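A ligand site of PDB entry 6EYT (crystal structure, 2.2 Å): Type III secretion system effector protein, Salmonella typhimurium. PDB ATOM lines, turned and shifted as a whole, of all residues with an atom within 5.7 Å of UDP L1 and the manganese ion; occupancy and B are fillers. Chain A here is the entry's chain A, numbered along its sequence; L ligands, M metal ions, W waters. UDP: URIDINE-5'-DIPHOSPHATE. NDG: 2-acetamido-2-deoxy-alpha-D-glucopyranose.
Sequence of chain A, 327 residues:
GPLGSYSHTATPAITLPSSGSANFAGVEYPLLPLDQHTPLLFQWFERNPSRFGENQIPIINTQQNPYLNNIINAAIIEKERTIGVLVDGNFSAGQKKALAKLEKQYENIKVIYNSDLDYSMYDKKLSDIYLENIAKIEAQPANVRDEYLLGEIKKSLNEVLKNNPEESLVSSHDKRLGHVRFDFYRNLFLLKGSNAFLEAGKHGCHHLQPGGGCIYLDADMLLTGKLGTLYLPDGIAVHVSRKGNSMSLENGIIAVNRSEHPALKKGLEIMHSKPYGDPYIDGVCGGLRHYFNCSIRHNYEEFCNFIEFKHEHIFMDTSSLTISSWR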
ATOM      1  N   PHE A  42      -9.647  13.826 -36.825  1.00  0.00           N
ATOM      2  CA  PHE A  42     -10.212  13.372 -35.575  1.00  0.00           C
ATOM      3  C   PHE A  42     -11.477  14.166 -35.311  1.00  0.00           C
ATOM      4  O   PHE A  42     -11.650  15.264 -35.843  1.00  0.00           O
ATOM      5  CB  PHE A  42      -9.223  13.526 -34.422  1.00  0.00           C
ATOM      6  CG  PHE A  42      -7.988  12.688 -34.574  1.00  0.00           C
ATOM      7  CD1 PHE A  42      -7.986  11.348 -34.194  1.00  0.00           C
ATOM      8  CD2 PHE A  42      -6.831  13.226 -35.115  1.00  0.00           C
ATOM      9  CE1 PHE A  42      -6.852  10.564 -34.346  1.00  0.00           C
ATOM     10  CE2 PHE A  42      -5.691  12.447 -35.271  1.00  0.00           C
ATOM     11  CZ  PHE A  42      -5.693  11.118 -34.885  1.00  0.00           C
ATOM     12  N   GLN A  43     -12.366  13.591 -34.500  1.00  0.00           N
ATOM     13  CA  GLN A  43     -13.631  14.230 -34.167  1.00  0.00           C
ATOM     14  C   GLN A  43     -13.847  14.185 -32.658  1.00  0.00           C
ATOM     15  O   GLN A  43     -13.661  13.137 -32.028  1.00  0.00           O
ATOM     16  CB  GLN A  43     -14.800  13.526 -34.871  1.00  0.00           C
ATOM     17  CG  GLN A  43     -16.161  14.140 -34.567  1.00  0.00           C
ATOM     18  CD  GLN A  43     -17.278  13.294 -35.119  1.00  0.00           C
ATOM     19  OE1 GLN A  43     -17.130  12.083 -35.252  1.00  0.00           O
ATOM     20  NE2 GLN A  43     -18.404  13.931 -35.450  1.00  0.00           N
ATOM     21  N   TRP A  44     -14.237  15.312 -32.078  1.00  0.00           N
ATOM     22  CA  TRP A  44     -14.647  15.317 -30.668  1.00  0.00           C
ATOM     23  C   TRP A  44     -15.860  16.225 -30.523  1.00  0.00           C
ATOM     24  O   TRP A  44     -15.726  17.450 -30.487  1.00  0.00           O
ATOM     25  CB  TRP A  44     -13.527  15.746 -29.740  1.00  0.00           C
ATOM     26  CG  TRP A  44     -13.965  15.549 -28.334  1.00  0.00           C
ATOM     27  CD1 TRP A  44     -14.263  16.524 -27.422  1.00  0.00           C
ATOM     28  CD2 TRP A  44     -14.235  14.300 -27.693  1.00  0.00           C
ATOM     29  NE1 TRP A  44     -14.682  15.949 -26.243  1.00  0.00           N
ATOM     30  CE2 TRP A  44     -14.679  14.584 -26.384  1.00  0.00           C
ATOM     31  CE3 TRP A  44     -14.146  12.967 -28.095  1.00  0.00           C
ATOM     32  CZ2 TRP A  44     -15.010  13.580 -25.471  1.00  0.00           C
ATOM     33  CZ3 TRP A  44     -14.481  11.971 -27.197  1.00  0.00           C
ATOM     34  CH2 TRP A  44     -14.912  12.285 -25.895  1.00  0.00           C
ATOM     35  N   PHE A  45     -17.046  15.609 -30.444  1.00  0.00           N
ATOM     36  CA  PHE A  45     -18.284  16.306 -30.126  1.00  0.00           C
ATOM     37  C   PHE A  45     -18.558  16.191 -28.634  1.00  0.00           C
ATOM     38  O   PHE A  45     -18.763  15.085 -28.120  1.00  0.00           O
ATOM     39  CB  PHE A  45     -19.461  15.728 -30.927  1.00  0.00           C
ATOM     40  CG  PHE A  45     -19.506  16.180 -32.354  1.00  0.00           C
ATOM     41  CD1 PHE A  45     -18.342  16.597 -32.997  1.00  0.00           C
ATOM     42  CD2 PHE A  45     -20.698  16.207 -33.046  1.00  0.00           C
ATOM     43  CE1 PHE A  45     -18.382  17.029 -34.322  1.00  0.00           C
ATOM     44  CE2 PHE A  45     -20.750  16.643 -34.359  1.00  0.00           C
ATOM     45  CZ  PHE A  45     -19.585  17.048 -34.996  1.00  0.00           C
ATOM     46  N   GLU A  46     -18.566  17.320 -27.940  1.00  0.00           N
ATOM     47  CA  GLU A  46     -18.741  17.341 -26.499  1.00  0.00           C
ATOM     48  C   GLU A  46     -20.145  17.844 -26.185  1.00  0.00           C
ATOM     49  O   GLU A  46     -20.481  19.000 -26.481  1.00  0.00           O
ATOM     50  CB  GLU A  46     -17.700  18.244 -25.829  1.00  0.00           C
ATOM     51  CG  GLU A  46     -17.849  18.337 -24.328  1.00  0.00           C
ATOM     52  CD  GLU A  46     -17.816  16.966 -23.663  1.00  0.00           C
ATOM     53  OE1 GLU A  46     -16.831  16.241 -23.885  1.00  0.00           O
ATOM     54  OE2 GLU A  46     -18.779  16.609 -22.956  1.00  0.00           O
ATOM     55  N   ARG A  47     -20.970  16.996 -25.576  1.00  0.00           N
ATOM     56  CA  ARG A  47     -22.320  17.412 -25.242  1.00  0.00           C
ATOM     57  C   ARG A  47     -22.412  18.042 -23.850  1.00  0.00           C
ATOM     58  O   ARG A  47     -23.456  18.610 -23.530  1.00  0.00           O
ATOM     59  CB  ARG A  47     -23.311  16.258 -25.368  1.00  0.00           C
ATOM     60  CG  ARG A  47     -22.838  14.884 -24.950  1.00  0.00           C
ATOM     61  CD  ARG A  47     -23.871  13.895 -25.474  1.00  0.00           C
ATOM     62  NE  ARG A  47     -23.694  12.536 -24.960  1.00  0.00           N
ATOM     63  CZ  ARG A  47     -22.815  11.673 -25.429  1.00  0.00           C
ATOM     64  NH1 ARG A  47     -22.002  12.016 -26.423  1.00  0.00           N
ATOM     65  NH2 ARG A  47     -22.736  10.448 -24.910  1.00  0.00           N
ATOM     66  N   ARG A  51     -18.012  20.089 -18.163  1.00  0.00           N
ATOM     67  CA  ARG A  51     -17.247  19.140 -17.373  1.00  0.00           C
ATOM     68  C   ARG A  51     -15.742  19.378 -17.485  1.00  0.00           C
ATOM     69  O   ARG A  51     -14.978  18.761 -16.728  1.00  0.00           O
ATOM     70  CB  ARG A  51     -17.572  17.699 -17.778  1.00  0.00           C
ATOM     71  CG  ARG A  51     -16.985  17.222 -19.109  1.00  0.00           C
ATOM     72  CD  ARG A  51     -17.678  15.935 -19.538  1.00  0.00           C
ATOM     73  NE  ARG A  51     -17.276  15.432 -20.850  1.00  0.00           N
ATOM     74  CZ  ARG A  51     -16.686  14.256 -21.055  1.00  0.00           C
ATOM     75  NH1 ARG A  51     -16.446  13.437 -20.048  1.00  0.00           N
ATOM     76  NH2 ARG A  51     -16.349  13.892 -22.293  1.00  0.00           N
ATOM     77  N   ASN A  65      -9.242   7.379 -21.252  1.00  0.00           N
ATOM     78  CA  ASN A  65      -9.457   7.799 -22.627  1.00  0.00           C
ATOM     79  C   ASN A  65      -8.568   9.001 -22.916  1.00  0.00           C
ATOM     80  O   ASN A  65      -9.033  10.148 -22.894  1.00  0.00           O
ATOM     81  CB  ASN A  65     -10.930   8.126 -22.887  1.00  0.00           C
ATOM     82  CG  ASN A  65     -11.836   6.933 -22.691  1.00  0.00           C
ATOM     83  OD1 ASN A  65     -12.406   6.733 -21.618  1.00  0.00           O
ATOM     84  ND2 ASN A  65     -11.986   6.122 -23.737  1.00  0.00           N
ATOM     85  N   TYR A  67      -7.539  10.805 -25.271  1.00  0.00           N
ATOM     86  CA  TYR A  67      -7.748  11.068 -26.694  1.00  0.00           C
ATOM     87  C   TYR A  67      -7.013  12.321 -27.152  1.00  0.00           C
ATOM     88  O   TYR A  67      -6.423  12.341 -28.242  1.00  0.00           O
ATOM     89  CB  TYR A  67      -9.249  11.172 -26.982  1.00  0.00           C
ATOM     90  CG  TYR A  67      -9.946   9.840 -26.841  1.00  0.00           C
ATOM     91  CD1 TYR A  67      -9.246   8.703 -26.470  1.00  0.00           C
ATOM     92  CD2 TYR A  67     -11.310   9.729 -27.066  1.00  0.00           C
ATOM     93  CE1 TYR A  67      -9.882   7.472 -26.330  1.00  0.00           C
ATOM     94  CE2 TYR A  67     -11.964   8.506 -26.937  1.00  0.00           C
ATOM     95  CZ  TYR A  67     -11.239   7.384 -26.557  1.00  0.00           C
ATOM     96  OH  TYR A  67     -11.871   6.172 -26.427  1.00  0.00           O
ATOM     97  N   PHE A 182     -22.981  12.714 -33.864  1.00  0.00           N
ATOM     98  CA  PHE A 182     -21.639  12.882 -34.393  1.00  0.00           C
ATOM     99  C   PHE A 182     -21.313  11.859 -35.473  1.00  0.00           C
ATOM    100  O   PHE A 182     -20.501  12.145 -36.356  1.00  0.00           O
ATOM    101  CB  PHE A 182     -20.575  12.913 -33.278  1.00  0.00           C
ATOM    102  CG  PHE A 182     -20.527  11.713 -32.380  1.00  0.00           C
ATOM    103  CD1 PHE A 182     -19.935  10.527 -32.800  1.00  0.00           C
ATOM    104  CD2 PHE A 182     -20.926  11.822 -31.050  1.00  0.00           C
ATOM    105  CE1 PHE A 182     -19.834   9.444 -31.932  1.00  0.00           C
ATOM    106  CE2 PHE A 182     -20.826  10.752 -30.188  1.00  0.00           C
ATOM    107  CZ  PHE A 182     -20.282   9.553 -30.623  1.00  0.00           C
ATOM    108  N   ARG A 186     -19.968  13.160 -39.105  1.00  0.00           N
ATOM    109  CA  ARG A 186     -18.730  12.552 -39.597  1.00  0.00           C
ATOM    110  C   ARG A 186     -18.859  12.234 -41.078  1.00  0.00           C
ATOM    111  O   ARG A 186     -17.947  12.517 -41.860  1.00  0.00           O
ATOM    112  CB  ARG A 186     -18.408  11.295 -38.792  1.00  0.00           C
ATOM    113  CG  ARG A 186     -17.102  10.586 -39.182  1.00  0.00           C
ATOM    114  CD  ARG A 186     -16.918   9.308 -38.374  1.00  0.00           C
ATOM    115  NE  ARG A 186     -16.986   9.575 -36.940  1.00  0.00           N
ATOM    116  CZ  ARG A 186     -17.107   8.632 -36.012  1.00  0.00           C
ATOM    117  NH1 ARG A 186     -17.162   7.345 -36.352  1.00  0.00           N
ATOM    118  NH2 ARG A 186     -17.161   8.977 -34.727  1.00  0.00           N
ATOM    119  N   TYR A 216     -10.338   9.659 -41.794  1.00  0.00           N
ATOM    120  CA  TYR A 216     -10.919   9.803 -40.467  1.00  0.00           C
ATOM    121  C   TYR A 216     -10.487   8.665 -39.557  1.00  0.00           C
ATOM    122  O   TYR A 216     -10.477   7.501 -39.967  1.00  0.00           O
ATOM    123  CB  TYR A 216     -12.450   9.845 -40.505  1.00  0.00           C
ATOM    124  CG  TYR A 216     -12.968   9.723 -39.104  1.00  0.00           C
ATOM    125  CD1 TYR A 216     -13.030  10.831 -38.280  1.00  0.00           C
ATOM    126  CD2 TYR A 216     -13.318   8.483 -38.574  1.00  0.00           C
ATOM    127  CE1 TYR A 216     -13.462  10.729 -36.971  1.00  0.00           C
ATOM    128  CE2 TYR A 216     -13.742   8.375 -37.264  1.00  0.00           C
ATOM    129  CZ  TYR A 216     -13.820   9.505 -36.471  1.00  0.00           C
ATOM    130  OH  TYR A 216     -14.240   9.398 -35.174  1.00  0.00           O
ATOM    131  N   LEU A 217     -10.177   8.992 -38.305  1.00  0.00           N
ATOM    132  CA  LEU A 217      -9.748   7.998 -37.341  1.00  0.00           C
ATOM    133  C   LEU A 217     -10.405   8.287 -36.010  1.00  0.00           C
ATOM    134  O   LEU A 217     -10.486   9.447 -35.591  1.00  0.00           O
ATOM    135  CB  LEU A 217      -8.220   7.982 -37.153  1.00  0.00           C
ATOM    136  CG  LEU A 217      -7.282   7.592 -38.301  1.00  0.00           C
ATOM    137  CD1 LEU A 217      -5.866   7.821 -37.862  1.00  0.00           C
ATOM    138  CD2 LEU A 217      -7.477   6.141 -38.737  1.00  0.00           C
ATOM    139  N   ASP A 218     -10.868   7.238 -35.339  1.00  0.00           N
ATOM    140  CA  ASP A 218     -11.288   7.394 -33.958  1.00  0.00           C
ATOM    141  C   ASP A 218     -10.084   7.795 -33.120  1.00  0.00           C
ATOM    142  O   ASP A 218      -8.954   7.341 -33.371  1.00  0.00           O
ATOM    143  CB  ASP A 218     -11.914   6.096 -33.438  1.00  0.00           C
ATOM    144  CG  ASP A 218     -13.404   6.023 -33.671  1.00  0.00           C
ATOM    145  OD1 ASP A 218     -13.979   7.017 -34.165  1.00  0.00           O
ATOM    146  OD2 ASP A 218     -14.011   4.961 -33.383  1.00  0.00           O
ATOM    147  N   ALA A 219     -10.307   8.656 -32.135  1.00  0.00           N
ATOM    148  CA  ALA A 219      -9.182   9.170 -31.356  1.00  0.00           C
ATOM    149  C   ALA A 219      -8.469   8.061 -30.609  1.00  0.00           C
ATOM    150  O   ALA A 219      -7.337   8.275 -30.140  1.00  0.00           O
ATOM    151  CB  ALA A 219      -9.661  10.254 -30.393  1.00  0.00           C
ATOM    152  N   ASP A 220      -9.082   6.887 -30.469  1.00  0.00           N
ATOM    153  CA  ASP A 220      -8.413   5.747 -29.856  1.00  0.00           C
ATOM    154  C   ASP A 220      -7.703   4.856 -30.879  1.00  0.00           C
ATOM    155  O   ASP A 220      -7.203   3.783 -30.497  1.00  0.00           O
ATOM    156  CB  ASP A 220      -9.418   4.916 -29.043  1.00  0.00           C
ATOM    157  CG  ASP A 220     -10.375   4.127 -29.935  1.00  0.00           C
ATOM    158  OD1 ASP A 220     -10.320   4.254 -31.175  1.00  0.00           O
ATOM    159  OD2 ASP A 220     -11.197   3.379 -29.378  1.00  0.00           O
ATOM    160  N   ASP A 317      -8.940   0.772 -32.226  1.00  0.00           N
ATOM    161  CA  ASP A 317      -9.997   0.722 -31.211  1.00  0.00           C
ATOM    162  C   ASP A 317      -9.457   0.356 -29.827  1.00  0.00           C
ATOM    163  O   ASP A 317      -9.902  -0.603 -29.184  1.00  0.00           O
ATOM    164  CB  ASP A 317     -11.112  -0.248 -31.630  1.00  0.00           C
ATOM    165  CG  ASP A 317     -12.365  -0.164 -30.734  1.00  0.00           C
ATOM    166  OD1 ASP A 317     -12.580   0.885 -30.093  1.00  0.00           O
ATOM    167  OD2 ASP A 317     -13.145  -1.133 -30.690  1.00  0.00           O
ATOM    168  N   THR A 318      -8.501   1.152 -29.356  1.00  0.00           N
ATOM    169  CA  THR A 318      -7.930   0.917 -28.036  1.00  0.00           C
ATOM    170  C   THR A 318      -8.900   1.193 -26.889  1.00  0.00           C
ATOM    171  O   THR A 318      -8.626   0.762 -25.757  1.00  0.00           O
ATOM    172  CB  THR A 318      -6.669   1.767 -27.828  1.00  0.00           C
ATOM    173  OG1 THR A 318      -6.999   3.159 -27.981  1.00  0.00           O
ATOM    174  CG2 THR A 318      -5.586   1.362 -28.811  1.00  0.00           C
ATOM    175  N   SER A 319     -10.035   1.849 -27.146  1.00  0.00           N
ATOM    176  CA  SER A 319     -11.006   2.048 -26.076  1.00  0.00           C
ATOM    177  C   SER A 319     -11.573   0.714 -25.611  1.00  0.00           C
ATOM    178  O   SER A 319     -11.939   0.568 -24.437  1.00  0.00           O
ATOM    179  CB  SER A 319     -12.146   2.950 -26.540  1.00  0.00           C
ATOM    180  OG  SER A 319     -12.918   2.306 -27.546  1.00  0.00           O
ATOM    181  N   SER A 320     -11.654  -0.268 -26.518  1.00  0.00           N
ATOM    182  CA  SER A 320     -12.126  -1.585 -26.135  1.00  0.00           C
ATOM    183  C   SER A 320     -11.204  -2.244 -25.110  1.00  0.00           C
ATOM    184  O   SER A 320     -11.627  -3.185 -24.437  1.00  0.00           O
ATOM    185  CB  SER A 320     -12.256  -2.457 -27.376  1.00  0.00           C
ATOM    186  OG  SER A 320     -10.987  -2.692 -27.953  1.00  0.00           O
ATOM    187  N   ILE A 323     -12.421   1.442 -21.636  1.00  0.00           N
ATOM    188  CA  ILE A 323     -13.865   1.704 -21.615  1.00  0.00           C
ATOM    189  C   ILE A 323     -14.166   2.677 -22.731  1.00  0.00           C
ATOM    190  O   ILE A 323     -13.349   3.539 -23.067  1.00  0.00           O
ATOM    191  CB  ILE A 323     -14.331   2.267 -20.247  1.00  0.00           C
ATOM    192  CG1 ILE A 323     -13.516   3.527 -19.883  1.00  0.00           C
ATOM    193  CG2 ILE A 323     -14.286   1.209 -19.155  1.00  0.00           C
ATOM    194  CD1 ILE A 323     -14.078   4.281 -18.703  1.00  0.00           C
ATOM    195  N   SER A 324     -15.351   2.531 -23.324  1.00  0.00           N
ATOM    196  CA  SER A 324     -15.834   3.506 -24.298  1.00  0.00           C
ATOM    197  C   SER A 324     -15.963   4.875 -23.637  1.00  0.00           C
ATOM    198  O   SER A 324     -16.189   4.991 -22.428  1.00  0.00           O
ATOM    199  CB  SER A 324     -17.175   3.076 -24.875  1.00  0.00           C
ATOM    200  OG  SER A 324     -17.790   4.130 -25.609  1.00  0.00           O
ATOM    201  N   SER A 325     -15.784   5.925 -24.438  1.00  0.00           N
ATOM    202  CA  SER A 325     -15.977   7.269 -23.909  1.00  0.00           C
ATOM    203  C   SER A 325     -17.443   7.694 -23.873  1.00  0.00           C
ATOM    204  O   SER A 325     -17.757   8.704 -23.242  1.00  0.00           O
ATOM    205  CB  SER A 325     -15.158   8.287 -24.721  1.00  0.00           C
ATOM    206  OG  SER A 325     -15.460   8.205 -26.102  1.00  0.00           O
ATOM    207  N   TRP A 326     -18.349   6.936 -24.518  1.00  0.00           N
ATOM    208  CA  TRP A 326     -19.754   7.339 -24.557  1.00  0.00           C
ATOM    209  C   TRP A 326     -20.749   6.211 -24.289  1.00  0.00           C
ATOM    210  O   TRP A 326     -21.929   6.512 -24.048  1.00  0.00           O
ATOM    211  CB  TRP A 326     -20.093   7.957 -25.919  1.00  0.00           C
ATOM    212  CG  TRP A 326     -19.968   7.001 -27.047  1.00  0.00           C
ATOM    213  CD1 TRP A 326     -18.830   6.698 -27.751  1.00  0.00           C
ATOM    214  CD2 TRP A 326     -21.011   6.220 -27.630  1.00  0.00           C
ATOM    215  NE1 TRP A 326     -19.113   5.776 -28.738  1.00  0.00           N
ATOM    216  CE2 TRP A 326     -20.449   5.463 -28.669  1.00  0.00           C
ATOM    217  CE3 TRP A 326     -22.376   6.084 -27.355  1.00  0.00           C
ATOM    218  CZ2 TRP A 326     -21.203   4.592 -29.448  1.00  0.00           C
ATOM    219  CZ3 TRP A 326     -23.120   5.211 -28.124  1.00  0.00           C
ATOM    220  CH2 TRP A 326     -22.534   4.482 -29.161  1.00  0.00           C
ATOM    221  N   ARG A 327     -20.346   4.942 -24.335  1.00  0.00           N
ATOM    222  CA  ARG A 327     -21.288   3.845 -24.063  1.00  0.00           C
ATOM    223  C   ARG A 327     -21.441   3.577 -22.572  1.00  0.00           C
ATOM    224  O   ARG A 327     -20.568   3.928 -21.766  1.00  0.00           O
ATOM    225  CB  ARG A 327     -20.847   2.552 -24.768  1.00  0.00           C
ATOM    226  CG  ARG A 327     -20.724   2.689 -26.277  1.00  0.00           C
ATOM    227  CD  ARG A 327     -20.194   1.407 -26.897  1.00  0.00           C
ATOM    228  NE  ARG A 327     -19.822   1.591 -28.301  1.00  0.00           N
ATOM    229  CZ  ARG A 327     -20.614   1.290 -29.329  1.00  0.00           C
ATOM    230  NH1 ARG A 327     -21.824   0.783 -29.102  1.00  0.00           N
ATOM    231  NH2 ARG A 327     -20.205   1.488 -30.565  1.00  0.00           N
HETATM  232  N1  UDP L   1     -16.932  10.760 -29.683  1.00  0.00           N
HETATM  233  C2  UDP L   1     -17.244  12.094 -29.603  1.00  0.00           C
HETATM  234  N3  UDP L   1     -17.750  12.503 -28.398  1.00  0.00           N
HETATM  235  C4  UDP L   1     -17.978  11.720 -27.281  1.00  0.00           C
HETATM  236  C5  UDP L   1     -17.620  10.347 -27.435  1.00  0.00           C
HETATM  237  C6  UDP L   1     -17.123   9.918 -28.615  1.00  0.00           C
HETATM  238  O2  UDP L   1     -17.089  12.877 -30.526  1.00  0.00           O
HETATM  239  O4  UDP L   1     -18.439  12.238 -26.250  1.00  0.00           O
HETATM  240  C1' UDP L   1     -16.372  10.264 -30.950  1.00  0.00           C
HETATM  241  C2' UDP L   1     -14.860  10.508 -31.066  1.00  0.00           C
HETATM  242  O2' UDP L   1     -14.534  10.837 -32.405  1.00  0.00           O
HETATM  243  C3' UDP L   1     -14.287   9.131 -30.709  1.00  0.00           C
HETATM  244  C4' UDP L   1     -15.327   8.208 -31.323  1.00  0.00           C
HETATM  245  O4' UDP L   1     -16.589   8.870 -31.038  1.00  0.00           O
HETATM  246  O3' UDP L   1     -13.014   8.944 -31.302  1.00  0.00           O
HETATM  247  C5' UDP L   1     -15.357   6.800 -30.784  1.00  0.00           C
HETATM  248  O5' UDP L   1     -15.075   6.836 -29.362  1.00  0.00           O
HETATM  249  PA  UDP L   1     -14.830   5.511 -28.535  1.00  0.00           P
HETATM  250  O1A UDP L   1     -13.754   4.751 -29.240  1.00  0.00           O
HETATM  251  O2A UDP L   1     -14.605   5.817 -27.051  1.00  0.00           O
HETATM  252  O3A UDP L   1     -16.211   4.715 -28.622  1.00  0.00           O
HETATM  253  PB  UDP L   1     -16.426   3.234 -29.164  1.00  0.00           P
HETATM  254  O1B UDP L   1     -15.211   2.695 -29.802  1.00  0.00           O
HETATM  255  O2B UDP L   1     -17.608   3.387 -30.133  1.00  0.00           O
HETATM  256  O3B UDP L   1     -16.876   2.482 -27.920  1.00  0.00           O
HETATM  257  C1  NDG L   2     -18.357   2.290 -33.498  1.00  0.00           C
HETATM  258  C2  NDG L   2     -17.211   3.231 -33.954  1.00  0.00           C
HETATM  259  C3  NDG L   2     -17.447   4.676 -33.454  1.00  0.00           C
HETATM  260  C4  NDG L   2     -18.886   5.105 -33.787  1.00  0.00           C
HETATM  261  C5  NDG L   2     -19.856   4.133 -33.108  1.00  0.00           C
HETATM  262  C6  NDG L   2     -21.332   4.485 -33.299  1.00  0.00           C
HETATM  263  C7  NDG L   2     -15.235   1.726 -34.257  1.00  0.00           C
HETATM  264  C8  NDG L   2     -13.923   1.220 -33.651  1.00  0.00           C
HETATM  265  O5  NDG L   2     -19.662   2.848 -33.726  1.00  0.00           O
HETATM  266  O3  NDG L   2     -16.524   5.576 -34.059  1.00  0.00           O
HETATM  267  O4  NDG L   2     -19.095   6.455 -33.373  1.00  0.00           O
HETATM  268  O6  NDG L   2     -21.768   4.255 -34.648  1.00  0.00           O
HETATM  269  O7  NDG L   2     -15.629   1.287 -35.347  1.00  0.00           O
HETATM  270  N2  NDG L   2     -15.928   2.671 -33.533  1.00  0.00           N
HETATM  271  O1  NDG L   2     -18.173   1.985 -32.139  1.00  0.00           O
HETATM  272 MN    MN M   1     -13.235   2.800 -29.592  1.00  0.00          MN
HETATM  273  O   HOH W   1     -11.901  10.919 -33.745  1.00  0.00           O
HETATM  274  O   HOH W   2     -12.164   6.786 -30.108  1.00  0.00           O
HETATM  275  O   HOH W   3     -19.490  14.308 -24.908  1.00  0.00           O
HETATM  276  O   HOH W   4     -12.702   3.089 -31.803  1.00  0.00           O
HETATM  277  O   HOH W   5     -15.339  -0.341 -29.598  1.00  0.00           O
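The manganese ion is bound by O1B of UDP L1 (2.0 Å), O1A of UDP L1 (2.0 Å), OD1 of Asp 317 (2.1 Å), OG of Ser 319 (2.1 Å), OD2 of Asp 220 (2.1 Å) and water W4 (2.3 Å). The manganese ion has six donor atoms within binding distance.
Water W4 lies within hydrogen-bond range of the side-chain carboxylate of Asp 220 (2.7 Å) and the side-chain carboxylate of Asp 218 (2.8 Å). Water W2 lies within hydrogen-bond range of O3' of UDP L1, N of Asp 220 and N of Ala 219. Water W1 lies within hydrogen-bond range of the backbone carbonyl oxygen of Leu 217 (2.8 Å), the backbone NH of Gln 43 (2.8 Å), an oxygen (O2') of UDP L1 (3.0 Å), the side-chain hydroxyl of Tyr 216 (3.1 Å) and the backbone NH of Ala 219 (3.2 Å).
Of the 25 residues printed, 3 come within 4 Å of the manganese ion. The nearest printed residue that does not touch the manganese ion is Asp 218 (4.4 Å).
O of Asp 317 is in hydrogen-bond range of OG of Ser 320 (2.7 Å). OG1 of Thr 318 lies within hydrogen-bond range of O of Asp 220 (2.6 Å). The side-chain amide nitrogen of Gln 43 lies within hydrogen-bond range of the backbone carbonyl oxygen of Phe 182 (2.9 Å). The side-chain amide oxygen (OE1) of Gln 43 lies within hydrogen-bond range of the guanidinium group (NE) of Arg 186 (3.0 Å). The side-chain amide nitrogen of Asn 65 lies within hydrogen-bond range of the side-chain hydroxyl of Tyr 67, 2.7 Å away. The backbone NH of Arg 327 is in hydrogen-bond range of the side-chain hydroxyl of Ser 324. OD1 of Asp 218 sits at hydrogen-bond distance from OH of Tyr 216 (2.6 Å). The guanidinium group (NH2) of Arg 186 lies within hydrogen-bond range of the side-chain hydroxyl (OH) of Tyr 216 (3.0 Å).
An oxygen (O2') of UDP L1 lies within hydrogen-bond range of the backbone carbonyl oxygen (O) of Gln 43, at 2.5 Å. N of Ser 325 sits at hydrogen-bond distance from O2A of UDP L1, 2.9 Å away. The side-chain hydroxyl (OG) of Ser 325 is in hydrogen-bond range of an oxygen (O2A) of UDP L1, 2.7 Å away. The backbone NH (N) of Phe 45 is in hydrogen-bond range of an oxygen (O2) of UDP L1, 2.7 Å away. The backbone carbonyl oxygen (O) of Phe 45 is in hydrogen-bond range of a nitrogen (N3) of UDP L1, at 2.8 Å. OH of Tyr 67 is in hydrogen-bond range of O2A of UDP L1 (2.8 Å). N of Ala 219 is in hydrogen-bond range of O3' of UDP L1 (2.8 Å). The side-chain hydroxyl (OG) of Ser 324 is in hydrogen-bond range of an oxygen (O3B) of UDP L1 (3.0 Å). NE1 of Trp 326 sits at hydrogen-bond distance from O3A of UDP L1 (3.1 Å). The guanidinium group (NE) of Arg 327 lies within salt-bridge range of an oxygen (O3B) of UDP L1, at 3.1 Å. An oxygen (O2') of UDP L1 lies within hydrogen-bond range of the side-chain hydroxyl (OH) of Tyr 216 (3.1 Å). O1 of NDG L2 sits at hydrogen-bond distance from NH2 of Arg 327 (2.6 Å). The side-chain carboxylate (OD2) of Asp 218 lies within hydrogen-bond range of an oxygen (O3) of NDG L2 (2.7 Å). O3 of NDG L2 lies within hydrogen-bond range of NH1 of Arg 186, 3.0 Å away.
An oxygen (O1) of NDG L2 sits at hydrogen-bond distance from an oxygen (O2B) of UDP L1 (2.5 Å).
Trp 44 touches UDP L1 (CH2 to C4, 3.4 Å). NH1 of Arg 47 touches O4 of UDP L1, 3.6 Å away. Phe 182 touches UDP L1. NH2 of Arg 186 touches O4' of UDP L1 (3.7 Å). OD1 of Asp 218 touches C4' of UDP L1, at 3.4 Å. Hydrophobic or aromatic side chains within 4 Å of UDP L1: Trp 44, Phe 45, Tyr 67, Phe 182, Ala 219 and Trp 326. Within 4 Å of UDP L1: Gln 43, Trp 44, Phe 45, Arg 47, Tyr 67, Phe 182, Arg 186, Tyr 216, Asp 218, Ala 219, Asp 220, Asp 317, Ser 319, Ser 324, Ser 325, Trp 326 and Arg 327.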
